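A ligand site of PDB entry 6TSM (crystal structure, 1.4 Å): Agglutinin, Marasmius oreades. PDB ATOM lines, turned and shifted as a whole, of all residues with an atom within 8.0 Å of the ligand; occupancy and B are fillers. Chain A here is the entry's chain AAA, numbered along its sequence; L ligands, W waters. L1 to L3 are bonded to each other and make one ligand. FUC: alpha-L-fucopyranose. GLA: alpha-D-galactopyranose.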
ATOM      1  N   ALA A  80      14.323   3.671 -36.819  1.00  0.00           N
ATOM      2  CA  ALA A  80      15.588   3.873 -36.095  1.00  0.00           C
ATOM      3  C   ALA A  80      16.608   4.536 -37.023  1.00  0.00           C
ATOM      4  O   ALA A  80      16.657   4.170 -38.218  1.00  0.00           O
ATOM      5  CB  ALA A  80      16.106   2.551 -35.562  1.00  0.00           C
ATOM      6  N   GLY A  81      17.239   5.602 -36.553  1.00  0.00           N
ATOM      7  CA  GLY A  81      18.293   6.307 -37.302  1.00  0.00           C
ATOM      8  C   GLY A  81      17.758   7.561 -37.979  1.00  0.00           C
ATOM      9  O   GLY A  81      18.505   8.200 -38.724  1.00  0.00           O
ATOM     10  N   LYS A 112      14.583  10.675 -20.377  1.00  0.00           N
ATOM     11  CA  LYS A 112      14.498  10.268 -21.786  1.00  0.00           C
ATOM     12  C   LYS A 112      13.603  11.260 -22.554  1.00  0.00           C
ATOM     13  O   LYS A 112      12.781  11.956 -21.906  1.00  0.00           O
ATOM     14  CB  LYS A 112      13.966   8.826 -21.898  1.00  0.00           C
ATOM     15  CG  LYS A 112      14.756   7.785 -21.112  1.00  0.00           C
ATOM     16  CD  LYS A 112      14.563   6.350 -21.608  1.00  0.00           C
ATOM     17  CE  LYS A 112      14.947   6.158 -23.075  1.00  0.00           C
ATOM     18  NZ  LYS A 112      15.266   4.742 -23.381  1.00  0.00           N
ATOM     19  N   PHE A 121      12.910   7.613 -29.424  1.00  0.00           N
ATOM     20  CA  PHE A 121      13.657   8.342 -28.393  1.00  0.00           C
ATOM     21  C   PHE A 121      14.900   8.995 -29.008  1.00  0.00           C
ATOM     22  O   PHE A 121      15.482   8.440 -29.931  1.00  0.00           O
ATOM     23  CB  PHE A 121      14.039   7.401 -27.261  1.00  0.00           C
ATOM     24  CG  PHE A 121      12.890   6.967 -26.393  1.00  0.00           C
ATOM     25  CD1 PHE A 121      12.504   7.716 -25.295  1.00  0.00           C
ATOM     26  CD2 PHE A 121      12.202   5.786 -26.655  1.00  0.00           C
ATOM     27  CE1 PHE A 121      11.438   7.325 -24.498  1.00  0.00           C
ATOM     28  CE2 PHE A 121      11.120   5.403 -25.857  1.00  0.00           C
ATOM     29  CZ  PHE A 121      10.766   6.157 -24.785  1.00  0.00           C
ATOM     30  N   VAL A 122      15.251  10.153 -28.511  1.00  0.00           N
ATOM     31  CA  VAL A 122      16.513  10.837 -28.873  1.00  0.00           C
ATOM     32  C   VAL A 122      17.707   9.971 -28.420  1.00  0.00           C
ATOM     33  O   VAL A 122      17.834   9.689 -27.198  1.00  0.00           O
ATOM     34  CB  VAL A 122      16.566  12.250 -28.270  1.00  0.00           C
ATOM     35  CG1 VAL A 122      17.882  12.937 -28.554  1.00  0.00           C
ATOM     36  CG2 VAL A 122      15.406  13.091 -28.762  1.00  0.00           C
ATOM     37  N   ASP A 123      18.588   9.653 -29.349  1.00  0.00           N
ATOM     38  CA  ASP A 123      19.617   8.625 -29.170  1.00  0.00           C
ATOM     39  C   ASP A 123      20.949   9.185 -29.692  1.00  0.00           C
ATOM     40  O   ASP A 123      21.015   9.525 -30.866  1.00  0.00           O
ATOM     41  CB  ASP A 123      19.193   7.325 -29.885  1.00  0.00           C
ATOM     42  CG  ASP A 123      20.133   6.151 -29.649  1.00  0.00           C
ATOM     43  OD1 ASP A 123      21.342   6.300 -29.929  1.00  0.00           O
ATOM     44  OD2 ASP A 123      19.635   5.068 -29.214  1.00  0.00           O
ATOM     45  N   LEU A 124      21.962   9.234 -28.845  1.00  0.00           N
ATOM     46  CA  LEU A 124      23.350   9.512 -29.280  1.00  0.00           C
ATOM     47  C   LEU A 124      23.932   8.236 -29.888  1.00  0.00           C
ATOM     48  O   LEU A 124      24.198   7.302 -29.127  1.00  0.00           O
ATOM     49  CB  LEU A 124      24.175   9.976 -28.093  1.00  0.00           C
ATOM     50  CG  LEU A 124      25.628  10.321 -28.399  1.00  0.00           C
ATOM     51  CD1 LEU A 124      25.731  11.498 -29.362  1.00  0.00           C
ATOM     52  CD2 LEU A 124      26.374  10.610 -27.127  1.00  0.00           C
ATOM     53  N   VAL A 125      23.956   8.156 -31.211  1.00  0.00           N
ATOM     54  CA  VAL A 125      24.077   6.833 -31.901  1.00  0.00           C
ATOM     55  C   VAL A 125      25.413   6.183 -31.509  1.00  0.00           C
ATOM     56  O   VAL A 125      26.466   6.850 -31.591  1.00  0.00           O
ATOM     57  CB  VAL A 125      23.931   7.001 -33.422  1.00  0.00           C
ATOM     58  CG1 VAL A 125      24.172   5.678 -34.136  1.00  0.00           C
ATOM     59  CG2 VAL A 125      22.576   7.576 -33.785  1.00  0.00           C
ATOM     60  N   ASN A 126      25.332   4.955 -30.982  1.00  0.00           N
ATOM     61  CA  ASN A 126      26.494   4.142 -30.584  1.00  0.00           C
ATOM     62  C   ASN A 126      27.205   4.779 -29.378  1.00  0.00           C
ATOM     63  O   ASN A 126      28.318   4.370 -29.075  1.00  0.00           O
ATOM     64  CB  ASN A 126      27.461   3.954 -31.748  1.00  0.00           C
ATOM     65  CG  ASN A 126      26.970   2.938 -32.720  1.00  0.00           C
ATOM     66  OD1 ASN A 126      26.367   1.927 -32.318  1.00  0.00           O
ATOM     67  ND2 ASN A 126      27.224   3.156 -33.992  1.00  0.00           N
ATOM     68  N   GLY A 127      26.589   5.746 -28.725  1.00  0.00           N
ATOM     69  CA  GLY A 127      27.226   6.418 -27.581  1.00  0.00           C
ATOM     70  C   GLY A 127      28.532   7.088 -27.999  1.00  0.00           C
ATOM     71  O   GLY A 127      29.460   7.152 -27.176  1.00  0.00           O
ATOM     72  N   ASP A 128      28.603   7.559 -29.231  1.00  0.00           N
ATOM     73  CA  ASP A 128      29.815   8.156 -29.825  1.00  0.00           C
ATOM     74  C   ASP A 128      30.097   9.501 -29.135  1.00  0.00           C
ATOM     75  O   ASP A 128      29.254  10.402 -29.240  1.00  0.00           O
ATOM     76  CB  ASP A 128      29.633   8.307 -31.325  1.00  0.00           C
ATOM     77  CG  ASP A 128      30.867   8.782 -32.064  1.00  0.00           C
ATOM     78  OD1 ASP A 128      31.854   9.104 -31.408  1.00  0.00           O
ATOM     79  OD2 ASP A 128      30.832   8.765 -33.310  1.00  0.00           O
ATOM     80  N   LYS A 134      26.292  11.771 -34.659  1.00  0.00           N
ATOM     81  CA  LYS A 134      24.856  11.773 -35.028  1.00  0.00           C
ATOM     82  C   LYS A 134      23.987  11.616 -33.765  1.00  0.00           C
ATOM     83  O   LYS A 134      24.261  10.675 -32.961  1.00  0.00           O
ATOM     84  CB  LYS A 134      24.576  10.652 -36.017  1.00  0.00           C
ATOM     85  CG  LYS A 134      23.134  10.508 -36.454  1.00  0.00           C
ATOM     86  CD  LYS A 134      22.959   9.455 -37.534  1.00  0.00           C
ATOM     87  CE  LYS A 134      21.578   9.438 -38.138  1.00  0.00           C
ATOM     88  NZ  LYS A 134      21.385   8.265 -39.043  1.00  0.00           N
ATOM     89  N   ALA A 136      19.850  10.738 -33.290  1.00  0.00           N
ATOM     90  CA  ALA A 136      18.765  10.199 -34.128  1.00  0.00           C
ATOM     91  C   ALA A 136      17.574   9.828 -33.271  1.00  0.00           C
ATOM     92  O   ALA A 136      17.759   9.606 -32.076  1.00  0.00           O
ATOM     93  CB  ALA A 136      19.263   9.013 -34.901  1.00  0.00           C
ATOM     94  N   GLY A 137      16.434   9.723 -33.869  1.00  0.00           N
ATOM     95  CA  GLY A 137      15.304   9.029 -33.274  1.00  0.00           C
ATOM     96  C   GLY A 137      15.497   7.517 -33.334  1.00  0.00           C
ATOM     97  O   GLY A 137      15.994   7.045 -34.336  1.00  0.00           O
ATOM     98  N   TRP A 138      15.289   6.833 -32.249  1.00  0.00           N
ATOM     99  CA  TRP A 138      15.604   5.377 -32.201  1.00  0.00           C
ATOM    100  C   TRP A 138      14.546   4.643 -31.371  1.00  0.00           C
ATOM    101  O   TRP A 138      14.041   5.214 -30.403  1.00  0.00           O
ATOM    102  CB  TRP A 138      17.021   5.165 -31.631  1.00  0.00           C
ATOM    103  CG  TRP A 138      17.677   3.935 -32.132  1.00  0.00           C
ATOM    104  CD1 TRP A 138      17.452   2.637 -31.730  1.00  0.00           C
ATOM    105  CD2 TRP A 138      18.724   3.870 -33.099  1.00  0.00           C
ATOM    106  NE1 TRP A 138      18.270   1.787 -32.397  1.00  0.00           N
ATOM    107  CE2 TRP A 138      19.067   2.503 -33.247  1.00  0.00           C
ATOM    108  CE3 TRP A 138      19.398   4.821 -33.866  1.00  0.00           C
ATOM    109  CZ2 TRP A 138      20.068   2.077 -34.122  1.00  0.00           C
ATOM    110  CZ3 TRP A 138      20.371   4.399 -34.738  1.00  0.00           C
ATOM    111  CH2 TRP A 138      20.701   3.042 -34.855  1.00  0.00           C
ATOM    112  N   THR A 139      14.284   3.394 -31.725  1.00  0.00           N
ATOM    113  CA  THR A 139      13.477   2.461 -30.905  1.00  0.00           C
ATOM    114  C   THR A 139      13.965   2.495 -29.474  1.00  0.00           C
ATOM    115  O   THR A 139      15.180   2.518 -29.290  1.00  0.00           O
ATOM    116  CB  THR A 139      13.565   1.035 -31.456  1.00  0.00           C
ATOM    117  OG1 THR A 139      13.604   1.097 -32.889  1.00  0.00           O
ATOM    118  CG2 THR A 139      12.406   0.168 -31.012  1.00  0.00           C
ATOM    119  N   GLY A 140      13.074   2.436 -28.529  1.00  0.00           N
ATOM    120  CA  GLY A 140      13.459   2.298 -27.116  1.00  0.00           C
ATOM    121  C   GLY A 140      12.293   2.116 -26.210  1.00  0.00           C
ATOM    122  O   GLY A 140      11.153   2.137 -26.707  1.00  0.00           O
ATOM    123  N   THR A 141      12.557   2.064 -24.914  1.00  0.00           N
ATOM    124  CA  THR A 141      11.487   1.975 -23.891  1.00  0.00           C
ATOM    125  C   THR A 141      11.738   3.012 -22.807  1.00  0.00           C
ATOM    126  O   THR A 141      12.932   3.408 -22.613  1.00  0.00           O
ATOM    127  CB  THR A 141      11.395   0.544 -23.293  1.00  0.00           C
ATOM    128  OG1 THR A 141      12.557   0.313 -22.514  1.00  0.00           O
ATOM    129  CG2 THR A 141      11.254  -0.523 -24.362  1.00  0.00           C
ATOM    130  N   GLU A 144      14.263   1.203 -19.718  1.00  0.00           N
ATOM    131  CA  GLU A 144      15.573   0.497 -19.949  1.00  0.00           C
ATOM    132  C   GLU A 144      16.750   1.396 -19.518  1.00  0.00           C
ATOM    133  O   GLU A 144      16.598   2.638 -19.555  1.00  0.00           O
ATOM    134  CB  GLU A 144      15.705   0.056 -21.401  1.00  0.00           C
ATOM    135  CG  GLU A 144      15.731   1.198 -22.387  1.00  0.00           C
ATOM    136  CD  GLU A 144      15.735   0.745 -23.835  1.00  0.00           C
ATOM    137  OE1 GLU A 144      16.008  -0.475 -24.081  1.00  0.00           O
ATOM    138  OE2 GLU A 144      15.482   1.595 -24.707  1.00  0.00           O
ATOM    139  N   GLY A 145      17.917   0.803 -19.269  1.00  0.00           N
ATOM    140  CA  GLY A 145      19.097   1.503 -18.719  1.00  0.00           C
ATOM    141  C   GLY A 145      19.951   2.171 -19.817  1.00  0.00           C
ATOM    142  O   GLY A 145      20.813   2.938 -19.470  1.00  0.00           O
ATOM    143  N   ASN A 146      19.680   1.855 -21.105  1.00  0.00           N
ATOM    144  CA  ASN A 146      20.511   2.262 -22.284  1.00  0.00           C
ATOM    145  C   ASN A 146      20.972   3.724 -22.135  1.00  0.00           C
ATOM    146  O   ASN A 146      20.181   4.631 -22.326  1.00  0.00           O
ATOM    147  CB  ASN A 146      19.743   2.050 -23.565  1.00  0.00           C
ATOM    148  CG  ASN A 146      20.539   2.409 -24.787  1.00  0.00           C
ATOM    149  OD1 ASN A 146      21.720   2.748 -24.695  1.00  0.00           O
ATOM    150  ND2 ASN A 146      19.909   2.296 -25.957  1.00  0.00           N
ATOM    151  N   PRO A 147      22.270   3.987 -21.891  1.00  0.00           N
ATOM    152  CA  PRO A 147      22.754   5.363 -21.697  1.00  0.00           C
ATOM    153  C   PRO A 147      22.748   6.193 -23.012  1.00  0.00           C
ATOM    154  O   PRO A 147      22.763   7.429 -22.915  1.00  0.00           O
ATOM    155  CB  PRO A 147      24.202   5.175 -21.177  1.00  0.00           C
ATOM    156  CG  PRO A 147      24.625   3.809 -21.750  1.00  0.00           C
ATOM    157  CD  PRO A 147      23.345   2.996 -21.800  1.00  0.00           C
ATOM    158  N   HIS A 148      22.704   5.527 -24.168  1.00  0.00           N
ATOM    159  CA  HIS A 148      22.595   6.257 -25.469  1.00  0.00           C
ATOM    160  C   HIS A 148      21.356   7.162 -25.453  1.00  0.00           C
ATOM    161  O   HIS A 148      21.340   8.161 -26.211  1.00  0.00           O
ATOM    162  CB  HIS A 148      22.550   5.295 -26.644  1.00  0.00           C
ATOM    163  CG  HIS A 148      23.708   4.374 -26.733  1.00  0.00           C
ATOM    164  ND1 HIS A 148      23.785   3.379 -27.708  1.00  0.00           N
ATOM    165  CD2 HIS A 148      24.868   4.292 -26.027  1.00  0.00           C
ATOM    166  CE1 HIS A 148      24.933   2.737 -27.590  1.00  0.00           C
ATOM    167  NE2 HIS A 148      25.608   3.260 -26.558  1.00  0.00           N
ATOM    168  N   GLN A 149      20.324   6.817 -24.664  1.00  0.00           N
ATOM    169  CA  GLN A 149      19.016   7.473 -24.724  1.00  0.00           C
ATOM    170  C   GLN A 149      18.708   8.193 -23.385  1.00  0.00           C
ATOM    171  O   GLN A 149      17.590   8.596 -23.207  1.00  0.00           O
ATOM    172  CB  GLN A 149      17.944   6.433 -25.055  1.00  0.00           C
ATOM    173  CG  GLN A 149      18.109   5.828 -26.438  1.00  0.00           C
ATOM    174  CD  GLN A 149      16.984   4.909 -26.832  1.00  0.00           C
ATOM    175  OE1 GLN A 149      16.010   4.707 -26.074  1.00  0.00           O
ATOM    176  NE2 GLN A 149      17.064   4.396 -28.044  1.00  0.00           N
HETATM  177  C1  FUC L   1      21.706  -1.555 -26.816  1.00  0.00           C
HETATM  178  C2  FUC L   1      21.353  -3.001 -26.473  1.00  0.00           C
HETATM  179  C3  FUC L   1      22.304  -3.960 -27.203  1.00  0.00           C
HETATM  180  C4  FUC L   1      23.713  -3.631 -26.821  1.00  0.00           C
HETATM  181  C5  FUC L   1      24.012  -2.163 -27.115  1.00  0.00           C
HETATM  182  C6  FUC L   1      25.423  -1.781 -26.701  1.00  0.00           C
HETATM  183  O2  FUC L   1      20.014  -3.277 -26.861  1.00  0.00           O
HETATM  184  O3  FUC L   1      22.011  -5.313 -26.832  1.00  0.00           O
HETATM  185  O4  FUC L   1      23.903  -3.906 -25.416  1.00  0.00           O
HETATM  186  O5  FUC L   1      23.039  -1.310 -26.411  1.00  0.00           O
HETATM  187  C1  GLA L   2      22.863   0.172 -29.564  1.00  0.00           C
HETATM  188  C2  GLA L   2      21.665   0.027 -28.591  1.00  0.00           C
HETATM  189  C3  GLA L   2      20.380   0.494 -29.237  1.00  0.00           C
HETATM  190  C4  GLA L   2      20.596   1.931 -29.732  1.00  0.00           C
HETATM  191  C5  GLA L   2      21.777   1.971 -30.703  1.00  0.00           C
HETATM  192  C6  GLA L   2      22.053   3.375 -31.268  1.00  0.00           C
HETATM  193  O1  GLA L   2      22.684  -0.691 -30.690  1.00  0.00           O
HETATM  194  O2  GLA L   2      21.550  -1.343 -28.165  1.00  0.00           O
HETATM  195  O3  GLA L   2      19.294   0.389 -28.290  1.00  0.00           O
HETATM  196  O4  GLA L   2      20.795   2.807 -28.602  1.00  0.00           O
HETATM  197  O5  GLA L   2      22.977   1.509 -30.031  1.00  0.00           O
HETATM  198  O6  GLA L   2      22.741   4.182 -30.297  1.00  0.00           O
HETATM  199  C1  GLA L   3      18.077   0.684 -28.693  1.00  0.00           C
HETATM  200  C2  GLA L   3      17.049   0.378 -27.699  1.00  0.00           C
HETATM  201  C3  GLA L   3      16.884  -1.143 -27.586  1.00  0.00           C
HETATM  202  C4  GLA L   3      16.539  -1.708 -28.928  1.00  0.00           C
HETATM  203  C5  GLA L   3      17.614  -1.261 -29.936  1.00  0.00           C
HETATM  204  C6  GLA L   3      17.330  -1.705 -31.358  1.00  0.00           C
HETATM  205  O2  GLA L   3      17.432   0.957 -26.414  1.00  0.00           O
HETATM  206  O3  GLA L   3      15.848  -1.432 -26.621  1.00  0.00           O
HETATM  207  O4  GLA L   3      15.233  -1.246 -29.342  1.00  0.00           O
HETATM  208  O5  GLA L   3      17.697   0.168 -29.932  1.00  0.00           O
HETATM  209  O6  GLA L   3      18.451  -1.347 -32.218  1.00  0.00           O
HETATM  210  O   HOH W   1      17.730  -0.548 -34.545  1.00  0.00           O
HETATM  211  O   HOH W   2      13.022  -1.268 -27.395  1.00  0.00           O
HETATM  212  O   HOH W   3      13.756  -3.191 -30.234  1.00  0.00           O
HETATM  213  O   HOH W   4      18.914  -1.250 -24.727  1.00  0.00           O
HETATM  214  O   HOH W   5      25.029  -1.603 -31.463  1.00  0.00           O
HETATM  215  O   HOH W   6      20.780  -2.975 -30.872  1.00  0.00           O
HETATM  216  O   HOH W   7      23.720   0.840 -24.788  1.00  0.00           O
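Residues that only touch the ligand: Thr 139, Val 125, Leu 124 and Gln 149. Hydrophobic or aromatic side chains within 4 Å of the ligand: Trp 138 and His 148. Ten residues have an atom within 4 Å of the ligand: Asp 123, Leu 124, Val 125, Asn 126, Trp 138, Thr 139, Glu 144, Asn 146, His 148 and Gln 149.
Water W1 lies within hydrogen-bond range of an oxygen (O6) of GLA L3 and the indole nitrogen of Trp 138. Water W7 lies within hydrogen-bond range of OD1 of Asn 146 (2.8 Å) and O5 of FUC L1 (2.8 Å). Water W4 bridges OE1 of Glu 144 and O2 of FUC L1.
NE2 of Gln 149 is in hydrogen-bond range of OD2 of Asp 123 (2.9 Å). N of His 148 sits at hydrogen-bond distance from OD1 of Asn 146 (3.0 Å). NE2 of His 148 sits at hydrogen-bond distance from N of Gly 127, at 3.4 Å. OE2 of Glu 144 is in salt-bridge range of NZ of Lys 112 (3.4 Å). O of His 148 lies within hydrogen-bond range of N of Leu 124 (2.9 Å). The side-chain amide oxygen of Gln 149 sits close to the side-chain carboxylate of Glu 144 (3.4 Å). The side-chain carboxylate (OD1) of Asp 123 lies close to the backbone NH (N) of Val 125. The backbone NH of Trp 138 is in hydrogen-bond range of the backbone carbonyl oxygen of Phe 121.
O6 of GLA L2 lies within hydrogen-bond range of OD1 of Asp 123 (2.6 Å). The side-chain amide nitrogen (ND2) of Asn 146 is in hydrogen-bond range of an oxygen (O4) of GLA L2. The indole nitrogen (NE1) of Trp 138 lies within hydrogen-bond range of an oxygen (O5) of GLA L3, at 3.0 Å. An oxygen (O6) of GLA L2 sits at hydrogen-bond distance from a ring nitrogen (ND1) of His 148 (2.9 Å). The side-chain carboxylate (OE2) of Glu 144 sits at hydrogen-bond distance from an oxygen (O2) of GLA L3 (2.7 Å). An oxygen (O6) of GLA L2 lies within hydrogen-bond range of the backbone NH of Asn 126 (2.8 Å).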
